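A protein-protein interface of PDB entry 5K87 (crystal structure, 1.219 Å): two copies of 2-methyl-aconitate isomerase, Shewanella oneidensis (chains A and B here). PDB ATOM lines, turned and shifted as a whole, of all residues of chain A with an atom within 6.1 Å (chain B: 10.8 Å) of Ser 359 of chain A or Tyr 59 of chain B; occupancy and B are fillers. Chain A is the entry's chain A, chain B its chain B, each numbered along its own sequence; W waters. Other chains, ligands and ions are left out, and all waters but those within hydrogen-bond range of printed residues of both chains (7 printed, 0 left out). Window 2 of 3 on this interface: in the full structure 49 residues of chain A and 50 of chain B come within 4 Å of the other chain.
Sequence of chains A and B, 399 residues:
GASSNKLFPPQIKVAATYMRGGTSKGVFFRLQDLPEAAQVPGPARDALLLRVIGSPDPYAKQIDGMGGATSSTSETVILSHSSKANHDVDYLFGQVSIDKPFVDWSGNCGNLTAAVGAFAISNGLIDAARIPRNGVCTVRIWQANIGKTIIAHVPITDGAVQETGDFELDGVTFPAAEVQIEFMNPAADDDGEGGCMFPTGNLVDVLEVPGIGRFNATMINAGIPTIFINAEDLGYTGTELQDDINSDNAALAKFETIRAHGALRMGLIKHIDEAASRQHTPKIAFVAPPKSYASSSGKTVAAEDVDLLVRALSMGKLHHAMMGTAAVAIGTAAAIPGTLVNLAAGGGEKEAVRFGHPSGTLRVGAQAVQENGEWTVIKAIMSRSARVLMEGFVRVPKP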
ATOM      1  N   LEU A 169     -20.139 -26.089  11.974  1.00  0.00           N
ATOM      2  CA  LEU A 169     -19.623 -24.903  11.298  1.00  0.00           C
ATOM      3  C   LEU A 169     -19.710 -23.770  12.299  1.00  0.00           C
ATOM      4  O   LEU A 169     -20.745 -23.624  12.953  1.00  0.00           O
ATOM      5  CB  LEU A 169     -20.517 -24.491  10.117  1.00  0.00           C
ATOM      6  CG  LEU A 169     -21.179 -25.380   9.068  1.00  0.00           C
ATOM      7  CD1 LEU A 169     -21.919 -24.523   8.054  1.00  0.00           C
ATOM      8  CD2 LEU A 169     -20.158 -26.190   8.363  1.00  0.00           C
ATOM      9  N   ASP A 170     -18.667 -22.949  12.398  1.00  0.00           N
ATOM     10  CA  ASP A 170     -18.741 -21.758  13.225  1.00  0.00           C
ATOM     11  C   ASP A 170     -19.746 -20.791  12.617  1.00  0.00           C
ATOM     12  O   ASP A 170     -19.674 -20.442  11.435  1.00  0.00           O
ATOM     13  CB  ASP A 170     -17.365 -21.105  13.385  1.00  0.00           C
ATOM     14  CG  ASP A 170     -16.450 -21.880  14.323  1.00  0.00           C
ATOM     15  OD1 ASP A 170     -16.933 -22.802  15.015  1.00  0.00           O
ATOM     16  OD2 ASP A 170     -15.244 -21.560  14.380  1.00  0.00           O
ATOM     17  N   GLY A 171     -20.708 -20.378  13.433  1.00  0.00           N
ATOM     18  CA  GLY A 171     -21.825 -19.581  12.965  1.00  0.00           C
ATOM     19  C   GLY A 171     -23.100 -20.388  12.784  1.00  0.00           C
ATOM     20  O   GLY A 171     -24.156 -19.809  12.525  1.00  0.00           O
ATOM     21  N   VAL A 172     -23.004 -21.713  12.888  1.00  0.00           N
ATOM     22  CA  VAL A 172     -24.184 -22.570  12.833  1.00  0.00           C
ATOM     23  C   VAL A 172     -24.340 -23.251  14.165  1.00  0.00           C
ATOM     24  O   VAL A 172     -23.461 -23.994  14.636  1.00  0.00           O
ATOM     25  CB  VAL A 172     -24.142 -23.603  11.709  1.00  0.00           C
ATOM     26  CG1 VAL A 172     -25.364 -24.526  11.792  1.00  0.00           C
ATOM     27  CG2 VAL A 172     -24.106 -22.898  10.363  1.00  0.00           C
ATOM     28  N   THR A 173     -25.492 -22.982  14.756  1.00  0.00           N
ATOM     29  CA  THR A 173     -25.761 -23.318  16.128  1.00  0.00           C
ATOM     30  C   THR A 173     -25.636 -24.826  16.404  1.00  0.00           C
ATOM     31  O   THR A 173     -25.019 -25.234  17.373  1.00  0.00           O
ATOM     32  CB  THR A 173     -27.158 -22.797  16.502  1.00  0.00           C
ATOM     33  OG1 THR A 173     -27.286 -21.417  16.077  1.00  0.00           O
ATOM     34  CG2 THR A 173     -27.388 -22.930  18.001  1.00  0.00           C
ATOM     35  N   LEU A 241     -16.110  -7.214  16.084  1.00  0.00           N
ATOM     36  CA  LEU A 241     -17.400  -7.896  16.003  1.00  0.00           C
ATOM     37  C   LEU A 241     -18.454  -6.926  15.472  1.00  0.00           C
ATOM     38  O   LEU A 241     -18.184  -5.737  15.323  1.00  0.00           O
ATOM     39  CB  LEU A 241     -17.793  -8.434  17.374  1.00  0.00           C
ATOM     40  CG  LEU A 241     -16.798  -9.430  17.970  1.00  0.00           C
ATOM     41  CD1 LEU A 241     -17.303  -9.948  19.309  1.00  0.00           C
ATOM     42  CD2 LEU A 241     -16.547 -10.573  16.997  1.00  0.00           C
ATOM     43  N   TYR A 293      -8.964 -13.583  19.634  1.00  0.00           N
ATOM     44  CA  TYR A 293     -10.163 -12.822  19.967  1.00  0.00           C
ATOM     45  C   TYR A 293     -11.296 -13.735  20.407  1.00  0.00           C
ATOM     46  O   TYR A 293     -11.313 -14.923  20.092  1.00  0.00           O
ATOM     47  CB  TYR A 293     -10.636 -11.973  18.781  1.00  0.00           C
ATOM     48  CG  TYR A 293     -11.080 -12.780  17.578  1.00  0.00           C
ATOM     49  CD1 TYR A 293     -10.144 -13.265  16.669  1.00  0.00           C
ATOM     50  CD2 TYR A 293     -12.430 -13.042  17.335  1.00  0.00           C
ATOM     51  CE1 TYR A 293     -10.526 -14.002  15.567  1.00  0.00           C
ATOM     52  CE2 TYR A 293     -12.825 -13.788  16.229  1.00  0.00           C
ATOM     53  CZ  TYR A 293     -11.866 -14.259  15.348  1.00  0.00           C
ATOM     54  OH  TYR A 293     -12.223 -14.991  14.241  1.00  0.00           O
ATOM     55  N   SER A 295     -14.989 -14.769  19.805  1.00  0.00           N
ATOM     56  CA  SER A 295     -15.970 -14.705  18.728  1.00  0.00           C
ATOM     57  C   SER A 295     -17.307 -14.256  19.289  1.00  0.00           C
ATOM     58  O   SER A 295     -17.479 -14.104  20.501  1.00  0.00           O
ATOM     59  CB  SER A 295     -16.140 -16.071  18.084  1.00  0.00           C
ATOM     60  OG  SER A 295     -16.914 -16.905  18.927  1.00  0.00           O
ATOM     61  N   SER A 296     -18.268 -14.058  18.398  1.00  0.00           N
ATOM     62  CA  SER A 296     -19.600 -13.620  18.790  1.00  0.00           C
ATOM     63  C   SER A 296     -20.328 -14.629  19.677  1.00  0.00           C
ATOM     64  O   SER A 296     -21.299 -14.279  20.343  1.00  0.00           O
ATOM     65  CB  SER A 296     -20.438 -13.339  17.547  1.00  0.00           C
ATOM     66  OG  SER A 296     -20.540 -14.507  16.760  1.00  0.00           O
ATOM     67  N   SER A 297     -19.884 -15.881  19.679  1.00  0.00           N
ATOM     68  CA  SER A 297     -20.497 -16.885  20.545  1.00  0.00           C
ATOM     69  C   SER A 297     -19.849 -16.939  21.922  1.00  0.00           C
ATOM     70  O   SER A 297     -20.344 -17.632  22.814  1.00  0.00           O
ATOM     71  CB  SER A 297     -20.410 -18.264  19.907  1.00  0.00           C
ATOM     72  OG  SER A 297     -19.071 -18.718  19.907  1.00  0.00           O
ATOM     73  N   LYS A 299     -16.697 -17.997  22.285  1.00  0.00           N
ATOM     74  CA  LYS A 299     -15.548 -18.891  22.143  1.00  0.00           C
ATOM     75  C   LYS A 299     -14.284 -18.139  21.744  1.00  0.00           C
ATOM     76  O   LYS A 299     -14.318 -17.239  20.902  1.00  0.00           O
ATOM     77  CB  LYS A 299     -15.822 -19.982  21.107  1.00  0.00           C
ATOM     78  CG  LYS A 299     -16.797 -21.059  21.544  1.00  0.00           C
ATOM     79  CD  LYS A 299     -16.814 -22.187  20.521  1.00  0.00           C
ATOM     80  CE  LYS A 299     -17.965 -23.151  20.752  1.00  0.00           C
ATOM     81  NZ  LYS A 299     -18.146 -24.066  19.586  1.00  0.00           N
ATOM     82  N   VAL A 301     -11.034 -17.631  19.729  1.00  0.00           N
ATOM     83  CA  VAL A 301     -10.287 -18.017  18.549  1.00  0.00           C
ATOM     84  C   VAL A 301      -8.841 -17.634  18.822  1.00  0.00           C
ATOM     85  O   VAL A 301      -8.522 -16.457  18.940  1.00  0.00           O
ATOM     86  CB  VAL A 301     -10.793 -17.265  17.303  1.00  0.00           C
ATOM     87  CG1 VAL A 301      -9.968 -17.635  16.082  1.00  0.00           C
ATOM     88  CG2 VAL A 301     -12.265 -17.573  17.055  1.00  0.00           C
ATOM     89  N   ARG A 311     -12.749  -9.762   7.931  1.00  0.00           N
ATOM     90  CA  ARG A 311     -14.094  -9.272   8.212  1.00  0.00           C
ATOM     91  C   ARG A 311     -14.633  -8.728   6.903  1.00  0.00           C
ATOM     92  O   ARG A 311     -13.900  -8.081   6.159  1.00  0.00           O
ATOM     93  CB  ARG A 311     -14.033  -8.153   9.243  1.00  0.00           C
ATOM     94  CG  ARG A 311     -14.326  -8.589  10.664  1.00  0.00           C
ATOM     95  CD  ARG A 311     -13.405  -9.682  11.176  1.00  0.00           C
ATOM     96  NE  ARG A 311     -13.630  -9.881  12.602  1.00  0.00           N
ATOM     97  CZ  ARG A 311     -13.197 -10.925  13.302  1.00  0.00           C
ATOM     98  NH1 ARG A 311     -12.486 -11.886  12.728  1.00  0.00           N
ATOM     99  NH2 ARG A 311     -13.464 -10.992  14.592  1.00  0.00           N
ATOM    100  N   HIS A 320     -22.126 -11.197   9.826  1.00  0.00           N
ATOM    101  CA  HIS A 320     -22.038 -11.887  11.108  1.00  0.00           C
ATOM    102  C   HIS A 320     -21.028 -13.029  11.104  1.00  0.00           C
ATOM    103  O   HIS A 320     -20.563 -13.462  12.162  1.00  0.00           O
ATOM    104  CB  HIS A 320     -23.421 -12.392  11.534  1.00  0.00           C
ATOM    105  CG  HIS A 320     -23.910 -13.575  10.756  1.00  0.00           C
ATOM    106  ND1 HIS A 320     -24.028 -14.828  11.316  1.00  0.00           N
ATOM    107  CD2 HIS A 320     -24.317 -13.699   9.468  1.00  0.00           C
ATOM    108  CE1 HIS A 320     -24.492 -15.670  10.411  1.00  0.00           C
ATOM    109  NE2 HIS A 320     -24.671 -15.014   9.279  1.00  0.00           N
ATOM    110  N   ALA A 321     -20.691 -13.528   9.920  1.00  0.00           N
ATOM    111  CA  ALA A 321     -19.757 -14.644   9.801  1.00  0.00           C
ATOM    112  C   ALA A 321     -18.911 -14.380   8.557  1.00  0.00           C
ATOM    113  O   ALA A 321     -18.145 -13.421   8.538  1.00  0.00           O
ATOM    114  CB  ALA A 321     -20.506 -15.970   9.736  1.00  0.00           C
ATOM    115  N   HIS A 357     -13.287 -15.075  11.279  1.00  0.00           N
ATOM    116  CA  HIS A 357     -14.355 -14.113  11.037  1.00  0.00           C
ATOM    117  C   HIS A 357     -15.101 -13.879  12.369  1.00  0.00           C
ATOM    118  O   HIS A 357     -14.732 -14.456  13.391  1.00  0.00           O
ATOM    119  CB  HIS A 357     -15.271 -14.617   9.908  1.00  0.00           C
ATOM    120  CG  HIS A 357     -15.865 -15.966  10.149  1.00  0.00           C
ATOM    121  ND1 HIS A 357     -16.887 -16.191  11.052  1.00  0.00           N
ATOM    122  CD2 HIS A 357     -15.599 -17.163   9.572  1.00  0.00           C
ATOM    123  CE1 HIS A 357     -17.215 -17.471  11.021  1.00  0.00           C
ATOM    124  NE2 HIS A 357     -16.452 -18.083  10.134  1.00  0.00           N
ATOM    125  N   PRO A 358     -16.125 -13.005  12.395  1.00  0.00           N
ATOM    126  CA  PRO A 358     -16.711 -12.710  13.711  1.00  0.00           C
ATOM    127  C   PRO A 358     -17.289 -13.904  14.463  1.00  0.00           C
ATOM    128  O   PRO A 358     -17.298 -13.874  15.689  1.00  0.00           O
ATOM    129  CB  PRO A 358     -17.794 -11.683  13.374  1.00  0.00           C
ATOM    130  CG  PRO A 358     -17.213 -10.951  12.219  1.00  0.00           C
ATOM    131  CD  PRO A 358     -16.594 -12.044  11.382  1.00  0.00           C
ATOM    132  N   SER A 359     -17.736 -14.937  13.758  1.00  0.00           N
ATOM    133  CA  SER A 359     -18.361 -16.082  14.420  1.00  0.00           C
ATOM    134  C   SER A 359     -17.419 -17.256  14.688  1.00  0.00           C
ATOM    135  O   SER A 359     -17.858 -18.275  15.222  1.00  0.00           O
ATOM    136  CB  SER A 359     -19.565 -16.581  13.607  1.00  0.00           C
ATOM    137  OG  SER A 359     -20.645 -15.666  13.683  1.00  0.00           O
ATOM    138  N   GLY A 360     -16.144 -17.122  14.326  1.00  0.00           N
ATOM    139  CA  GLY A 360     -15.207 -18.225  14.472  1.00  0.00           C
ATOM    140  C   GLY A 360     -14.333 -18.361  13.248  1.00  0.00           C
ATOM    141  O   GLY A 360     -13.841 -17.363  12.718  1.00  0.00           O
ATOM    142  N   THR A 361     -14.129 -19.585  12.782  1.00  0.00           N
ATOM    143  CA  THR A 361     -13.177 -19.791  11.698  1.00  0.00           C
ATOM    144  C   THR A 361     -13.805 -20.523  10.519  1.00  0.00           C
ATOM    145  O   THR A 361     -14.856 -21.148  10.652  1.00  0.00           O
ATOM    146  CB  THR A 361     -11.920 -20.555  12.165  1.00  0.00           C
ATOM    147  OG1 THR A 361     -12.243 -21.934  12.356  1.00  0.00           O
ATOM    148  CG2 THR A 361     -11.387 -19.978  13.464  1.00  0.00           C
ATOM    149  N   GLY B  54     -34.712 -22.363  16.953  1.00  0.00           N
ATOM    150  CA  GLY B  54     -33.278 -22.249  16.748  1.00  0.00           C
ATOM    151  C   GLY B  54     -32.507 -21.827  17.986  1.00  0.00           C
ATOM    152  O   GLY B  54     -31.435 -21.238  17.875  1.00  0.00           O
ATOM    153  N   SER B  55     -33.044 -22.149  19.160  1.00  0.00           N
ATOM    154  CA  SER B  55     -32.481 -21.753  20.448  1.00  0.00           C
ATOM    155  C   SER B  55     -32.092 -22.976  21.292  1.00  0.00           C
ATOM    156  O   SER B  55     -32.564 -24.070  21.028  1.00  0.00           O
ATOM    157  CB  SER B  55     -33.523 -20.959  21.236  1.00  0.00           C
ATOM    158  OG  SER B  55     -33.723 -19.654  20.723  1.00  0.00           O
ATOM    159  N   PRO B  56     -31.238 -22.786  22.315  1.00  0.00           N
ATOM    160  CA  PRO B  56     -30.508 -21.555  22.625  1.00  0.00           C
ATOM    161  C   PRO B  56     -29.423 -21.324  21.593  1.00  0.00           C
ATOM    162  O   PRO B  56     -28.823 -22.278  21.081  1.00  0.00           O
ATOM    163  CB  PRO B  56     -29.895 -21.844  24.003  1.00  0.00           C
ATOM    164  CG  PRO B  56     -29.735 -23.309  24.036  1.00  0.00           C
ATOM    165  CD  PRO B  56     -30.865 -23.892  23.220  1.00  0.00           C
ATOM    166  N   ASP B  57     -29.181 -20.062  21.279  1.00  0.00           N
ATOM    167  CA  ASP B  57     -28.219 -19.746  20.239  1.00  0.00           C
ATOM    168  C   ASP B  57     -27.182 -18.774  20.753  1.00  0.00           C
ATOM    169  O   ASP B  57     -27.470 -17.596  20.907  1.00  0.00           O
ATOM    170  CB  ASP B  57     -28.913 -19.141  19.022  1.00  0.00           C
ATOM    171  CG  ASP B  57     -27.936 -18.818  17.917  1.00  0.00           C
ATOM    172  OD1 ASP B  57     -26.840 -19.414  17.914  1.00  0.00           O
ATOM    173  OD2 ASP B  57     -28.260 -17.981  17.052  1.00  0.00           O
ATOM    174  N   PRO B  58     -25.955 -19.253  21.000  1.00  0.00           N
ATOM    175  CA  PRO B  58     -24.916 -18.339  21.489  1.00  0.00           C
ATOM    176  C   PRO B  58     -24.547 -17.243  20.475  1.00  0.00           C
ATOM    177  O   PRO B  58     -23.996 -16.218  20.868  1.00  0.00           O
ATOM    178  CB  PRO B  58     -23.724 -19.263  21.772  1.00  0.00           C
ATOM    179  CG  PRO B  58     -23.961 -20.472  20.969  1.00  0.00           C
ATOM    180  CD  PRO B  58     -25.461 -20.626  20.810  1.00  0.00           C
ATOM    181  N   TYR B  59     -24.881 -17.435  19.203  1.00  0.00           N
ATOM    182  CA  TYR B  59     -24.623 -16.411  18.186  1.00  0.00           C
ATOM    183  C   TYR B  59     -25.698 -15.323  18.163  1.00  0.00           C
ATOM    184  O   TYR B  59     -25.511 -14.271  17.536  1.00  0.00           O
ATOM    185  CB  TYR B  59     -24.546 -17.033  16.799  1.00  0.00           C
ATOM    186  CG  TYR B  59     -23.473 -18.076  16.665  1.00  0.00           C
ATOM    187  CD1 TYR B  59     -22.130 -17.719  16.583  1.00  0.00           C
ATOM    188  CD2 TYR B  59     -23.799 -19.425  16.606  1.00  0.00           C
ATOM    189  CE1 TYR B  59     -21.142 -18.683  16.460  1.00  0.00           C
ATOM    190  CE2 TYR B  59     -22.814 -20.396  16.494  1.00  0.00           C
ATOM    191  CZ  TYR B  59     -21.490 -20.016  16.410  1.00  0.00           C
ATOM    192  OH  TYR B  59     -20.521 -20.988  16.286  1.00  0.00           O
ATOM    193  N   ALA B  60     -26.836 -15.593  18.807  1.00  0.00           N
ATOM    194  CA  ALA B  60     -27.959 -14.654  18.870  1.00  0.00           C
ATOM    195  C   ALA B  60     -28.481 -14.251  17.498  1.00  0.00           C
ATOM    196  O   ALA B  60     -28.845 -13.096  17.286  1.00  0.00           O
ATOM    197  CB  ALA B  60     -27.595 -13.413  19.694  1.00  0.00           C
ATOM    198  N   LYS B  61     -28.513 -15.203  16.572  1.00  0.00           N
ATOM    199  CA  LYS B  61     -29.019 -14.954  15.220  1.00  0.00           C
ATOM    200  C   LYS B  61     -30.168 -15.863  14.806  1.00  0.00           C
ATOM    201  O   LYS B  61     -30.871 -15.548  13.849  1.00  0.00           O
ATOM    202  CB  LYS B  61     -27.902 -15.089  14.187  1.00  0.00           C
ATOM    203  CG  LYS B  61     -26.778 -14.080  14.338  1.00  0.00           C
ATOM    204  CD  LYS B  61     -27.267 -12.673  14.068  1.00  0.00           C
ATOM    205  CE  LYS B  61     -26.137 -11.676  14.191  1.00  0.00           C
ATOM    206  NZ  LYS B  61     -26.622 -10.272  14.079  1.00  0.00           N
ATOM    207  N   GLN B  62     -30.344 -16.992  15.495  1.00  0.00           N
ATOM    208  CA  GLN B  62     -31.367 -17.982  15.135  1.00  0.00           C
ATOM    209  C   GLN B  62     -31.346 -18.358  13.648  1.00  0.00           C
ATOM    210  O   GLN B  62     -32.381 -18.501  13.003  1.00  0.00           O
ATOM    211  CB  GLN B  62     -32.760 -17.562  15.629  1.00  0.00           C
ATOM    212  CG  GLN B  62     -32.832 -17.585  17.158  1.00  0.00           C
ATOM    213  CD  GLN B  62     -34.136 -17.071  17.742  1.00  0.00           C
ATOM    214  OE1 GLN B  62     -34.828 -16.239  17.151  1.00  0.00           O
ATOM    215  NE2 GLN B  62     -34.467 -17.552  18.930  1.00  0.00           N
ATOM    216  N   ILE B  63     -30.140 -18.537  13.117  1.00  0.00           N
ATOM    217  CA  ILE B  63     -29.958 -18.894  11.713  1.00  0.00           C
ATOM    218  C   ILE B  63     -30.308 -20.369  11.488  1.00  0.00           C
ATOM    219  O   ILE B  63     -30.517 -20.801  10.361  1.00  0.00           O
ATOM    220  CB  ILE B  63     -28.512 -18.580  11.255  1.00  0.00           C
ATOM    221  CG1 ILE B  63     -28.310 -17.074  11.178  1.00  0.00           C
ATOM    222  CG2 ILE B  63     -28.193 -19.173   9.887  1.00  0.00           C
ATOM    223  CD1 ILE B  63     -28.935 -16.491   9.976  1.00  0.00           C
ATOM    224  N   ASP B  64     -30.385 -21.140  12.567  1.00  0.00           N
ATOM    225  CA  ASP B  64     -30.691 -22.558  12.440  1.00  0.00           C
ATOM    226  C   ASP B  64     -32.075 -22.887  12.995  1.00  0.00           C
ATOM    227  O   ASP B  64     -32.276 -23.927  13.622  1.00  0.00           O
ATOM    228  CB  ASP B  64     -29.608 -23.385  13.119  1.00  0.00           C
ATOM    229  CG  ASP B  64     -29.515 -24.798  12.584  1.00  0.00           C
ATOM    230  OD1 ASP B  64     -30.110 -25.118  11.545  1.00  0.00           O
ATOM    231  OD2 ASP B  64     -28.787 -25.583  13.239  1.00  0.00           O
ATOM    232  N   GLY B  65     -33.042 -21.999  12.777  1.00  0.00           N
ATOM    233  CA  GLY B  65     -34.416 -22.249  13.184  1.00  0.00           C
ATOM    234  C   GLY B  65     -35.339 -21.200  12.605  1.00  0.00           C
ATOM    235  O   GLY B  65     -34.915 -20.360  11.800  1.00  0.00           O
ATOM    236  N   GLY B  68     -36.406 -15.152  14.487  1.00  0.00           N
ATOM    237  CA  GLY B  68     -35.828 -13.997  13.822  1.00  0.00           C
ATOM    238  C   GLY B  68     -34.889 -13.225  14.725  1.00  0.00           C
ATOM    239  O   GLY B  68     -34.517 -12.090  14.401  1.00  0.00           O
ATOM    240  N   ALA B  69     -34.513 -13.818  15.855  1.00  0.00           N
ATOM    241  CA  ALA B  69     -33.513 -13.259  16.766  1.00  0.00           C
ATOM    242  C   ALA B  69     -33.958 -11.974  17.457  1.00  0.00           C
ATOM    243  O   ALA B  69     -33.125 -11.156  17.847  1.00  0.00           O
ATOM    244  CB  ALA B  69     -32.170 -13.057  16.055  1.00  0.00           C
ATOM    245  N   THR B  70     -35.265 -11.800  17.608  1.00  0.00           N
ATOM    246  CA  THR B  70     -35.806 -10.714  18.417  1.00  0.00           C
ATOM    247  C   THR B  70     -36.930 -11.305  19.246  1.00  0.00           C
ATOM    248  O   THR B  70     -37.481 -12.354  18.893  1.00  0.00           O
ATOM    249  CB  THR B  70     -36.373  -9.558  17.575  1.00  0.00           C
ATOM    250  OG1 THR B  70     -37.560  -9.995  16.917  1.00  0.00           O
ATOM    251  CG2 THR B  70     -35.357  -9.045  16.562  1.00  0.00           C
ATOM    252  N   SER B  97     -36.676 -18.224  24.675  1.00  0.00           N
ATOM    253  CA  SER B  97     -35.454 -17.485  24.925  1.00  0.00           C
ATOM    254  C   SER B  97     -34.505 -17.601  23.740  1.00  0.00           C
ATOM    255  O   SER B  97     -34.401 -18.658  23.128  1.00  0.00           O
ATOM    256  CB  SER B  97     -34.772 -18.028  26.175  1.00  0.00           C
ATOM    257  OG  SER B  97     -33.571 -17.336  26.414  1.00  0.00           O
ATOM    258  N   ILE B  98     -33.821 -16.514  23.416  1.00  0.00           N
ATOM    259  CA  ILE B  98     -32.815 -16.568  22.372  1.00  0.00           C
ATOM    260  C   ILE B  98     -31.540 -17.238  22.871  1.00  0.00           C
ATOM    261  O   ILE B  98     -30.942 -18.042  22.163  1.00  0.00           O
ATOM    262  CB  ILE B  98     -32.523 -15.163  21.821  1.00  0.00           C
ATOM    263  CG1 ILE B  98     -33.799 -14.600  21.182  1.00  0.00           C
ATOM    264  CG2 ILE B  98     -31.395 -15.205  20.801  1.00  0.00           C
ATOM    265  CD1 ILE B  98     -33.730 -13.123  20.844  1.00  0.00           C
ATOM    266  N   ASP B  99     -31.140 -16.903  24.095  1.00  0.00           N
ATOM    267  CA  ASP B  99     -29.840 -17.308  24.623  1.00  0.00           C
ATOM    268  C   ASP B  99     -29.874 -18.470  25.621  1.00  0.00           C
ATOM    269  O   ASP B  99     -28.844 -19.100  25.852  1.00  0.00           O
ATOM    270  CB  ASP B  99     -29.122 -16.103  25.246  1.00  0.00           C
ATOM    271  CG  ASP B  99     -29.876 -15.512  26.414  1.00  0.00           C
ATOM    272  OD1 ASP B  99     -31.112 -15.380  26.329  1.00  0.00           O
ATOM    273  OD2 ASP B  99     -29.228 -15.173  27.428  1.00  0.00           O
ATOM    274  N   LYS B 100     -31.034 -18.750  26.213  1.00  0.00           N
ATOM    275  CA  LYS B 100     -31.137 -19.776  27.256  1.00  0.00           C
ATOM    276  C   LYS B 100     -32.000 -20.924  26.774  1.00  0.00           C
ATOM    277  O   LYS B 100     -32.879 -20.726  25.944  1.00  0.00           O
ATOM    278  CB  LYS B 100     -31.767 -19.188  28.522  1.00  0.00           C
ATOM    279  CG  LYS B 100     -31.075 -17.954  29.051  1.00  0.00           C
ATOM    280  CD  LYS B 100     -29.623 -18.230  29.375  1.00  0.00           C
ATOM    281  CE  LYS B 100     -28.989 -17.047  30.102  1.00  0.00           C
ATOM    282  NZ  LYS B 100     -29.603 -16.844  31.444  1.00  0.00           N
ATOM    283  N   LYS B 317     -34.596  -5.648  25.770  1.00  0.00           N
ATOM    284  CA  LYS B 317     -34.362  -4.683  24.701  1.00  0.00           C
ATOM    285  C   LYS B 317     -35.574  -3.784  24.540  1.00  0.00           C
ATOM    286  O   LYS B 317     -36.702  -4.208  24.774  1.00  0.00           O
ATOM    287  CB  LYS B 317     -34.123  -5.403  23.370  1.00  0.00           C
ATOM    288  CG  LYS B 317     -32.847  -6.213  23.307  1.00  0.00           C
ATOM    289  CD  LYS B 317     -31.649  -5.289  23.224  1.00  0.00           C
ATOM    290  CE  LYS B 317     -30.341  -6.057  23.291  1.00  0.00           C
ATOM    291  NZ  LYS B 317     -30.210  -7.009  22.157  1.00  0.00           N
HETATM  292  O   HOH W   1     -27.556 -18.620  14.481  1.00  0.00           O
HETATM  293  O   HOH W   2     -30.001 -21.003  15.450  1.00  0.00           O
HETATM  294  O   HOH W   3     -23.375 -13.706  15.738  1.00  0.00           O
HETATM  295  O   HOH W   4     -26.958 -20.914  13.072  1.00  0.00           O
HETATM  296  O   HOH W   5     -23.756 -13.257  20.786  1.00  0.00           O
HETATM  297  O   HOH W   6     -18.818 -20.883  18.357  1.00  0.00           O
HETATM  298  O   HOH W   7     -21.281 -23.595  16.227  1.00  0.00           O
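Ser 359 of chain A touches just one residue of chain B: Tyr 59.
Of chain A, only Asp 170 (3.6 Å), Gly 171 (2.9 Å), Val 172 (3.8 Å), Ser 296 (3.6 Å), Ser 297 (3.5 Å) and Ser 359 (3.5 Å) come within 4 Å of Tyr 59 of chain B.
Thr 173 of chain A touches just these residues of chain B: Pro 56 (3.5 Å) and Asp 57 (2.8 Å).
Ser 295 of chain A touches none of the printed residues of chain B.
Of chain B, only Pro 58 and Tyr 59 come within 4 Å of Ser 296 of chain A.
Printed residues of chain B within 4 Å of His 320 of chain A: Lys 61.
Ala 321 of chain A touches none of the printed residues of chain B.
No residue of chain B comes within 4 Å of His 357 of chain A.
Pro 358 of chain A touches none of the printed residues of chain B.
Of the printed residues of chain A, Lys 61 of chain B touches His 320 (3.9 Å).
Of the printed residues of chain A, Asp 57 of chain B touches Thr 173.
The nearest residue of chain A that does not touch Tyr 59 of chain B is Thr 173 of chain A (4.1 Å).
The backbone NH of Asp 57 of chain B sits at hydrogen-bond distance from the backbone carbonyl oxygen of Ile 98 of chain B (2.8 Å).
The side-chain hydroxyl of Ser 295 of chain A sits at hydrogen-bond distance from the side-chain hydroxyl of Ser 297 of chain A (3.0 Å).
N of Ser 296 of chain A is in hydrogen-bond range of O of Pro 358 of chain A (2.9 Å).
OD2 of Asp 57 of chain B is in hydrogen-bond range of N of Lys 61 of chain B (2.8 Å).
Tyr 59 of chain B touches Asp 170 of chain A.
N of Val 172 of chain A touches CE2 of Tyr 59 of chain B (3.8 Å).
Val 172 of chain A touches Asp 64 of chain B.
Thr 173 of chain A touches Pro 56 of chain B.
Tyr 59 of chain B touches Ser 296 of chain A (CD1 to OG, 3.6 Å).
Ser 297 of chain A touches Tyr 59 of chain B.
Lys 61 of chain B touches His 320 of chain A (CE to CB, 3.9 Å).
Ser 359 of chain A touches Tyr 59 of chain B (O to CE1, 3.5 Å).
The side-chain hydroxyl (OH) of Tyr 59 of chain B is in hydrogen-bond range of the backbone NH (N) of Gly 171 of chain A (2.9 Å).
O of Ser 296 of chain A lies close to O of Pro 58 of chain B (3.4 Å).
The side-chain hydroxyl of Thr 173 of chain A sits at hydrogen-bond distance from the side-chain carboxylate of Asp 57 of chain B, 2.8 Å away.
No position is printed for both chains.
Of the 12 pairs that touch across the chains among the printed residues, none has its exchanged pair printed and touching as well.
Printed residues of chain A that touch a printed residue of chain B: Asp 170, Gly 171, Val 172, Thr 173, Ser 296, Ser 297, His 320 and Ser 359.
Hydrophobic or aromatic side chains of chain A within 4 Å of the printed part of chain B: Val 172 and His 320.
Among the printed residues, no Asp or Glu carboxylate lies within 4 Å of a Lys or Arg side-chain nitrogen of the other chain.
Water W5 bridges O of Ser 296 of chain A and O of Pro 58 of chain B.
Water W7 lies within hydrogen-bond range of the side-chain hydroxyl of Tyr 59 of chain B (2.7 Å), the backbone carbonyl oxygen of Val 172 of chain A (2.7 Å) and the backbone carbonyl oxygen of Leu 169 of chain A (3.3 Å).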
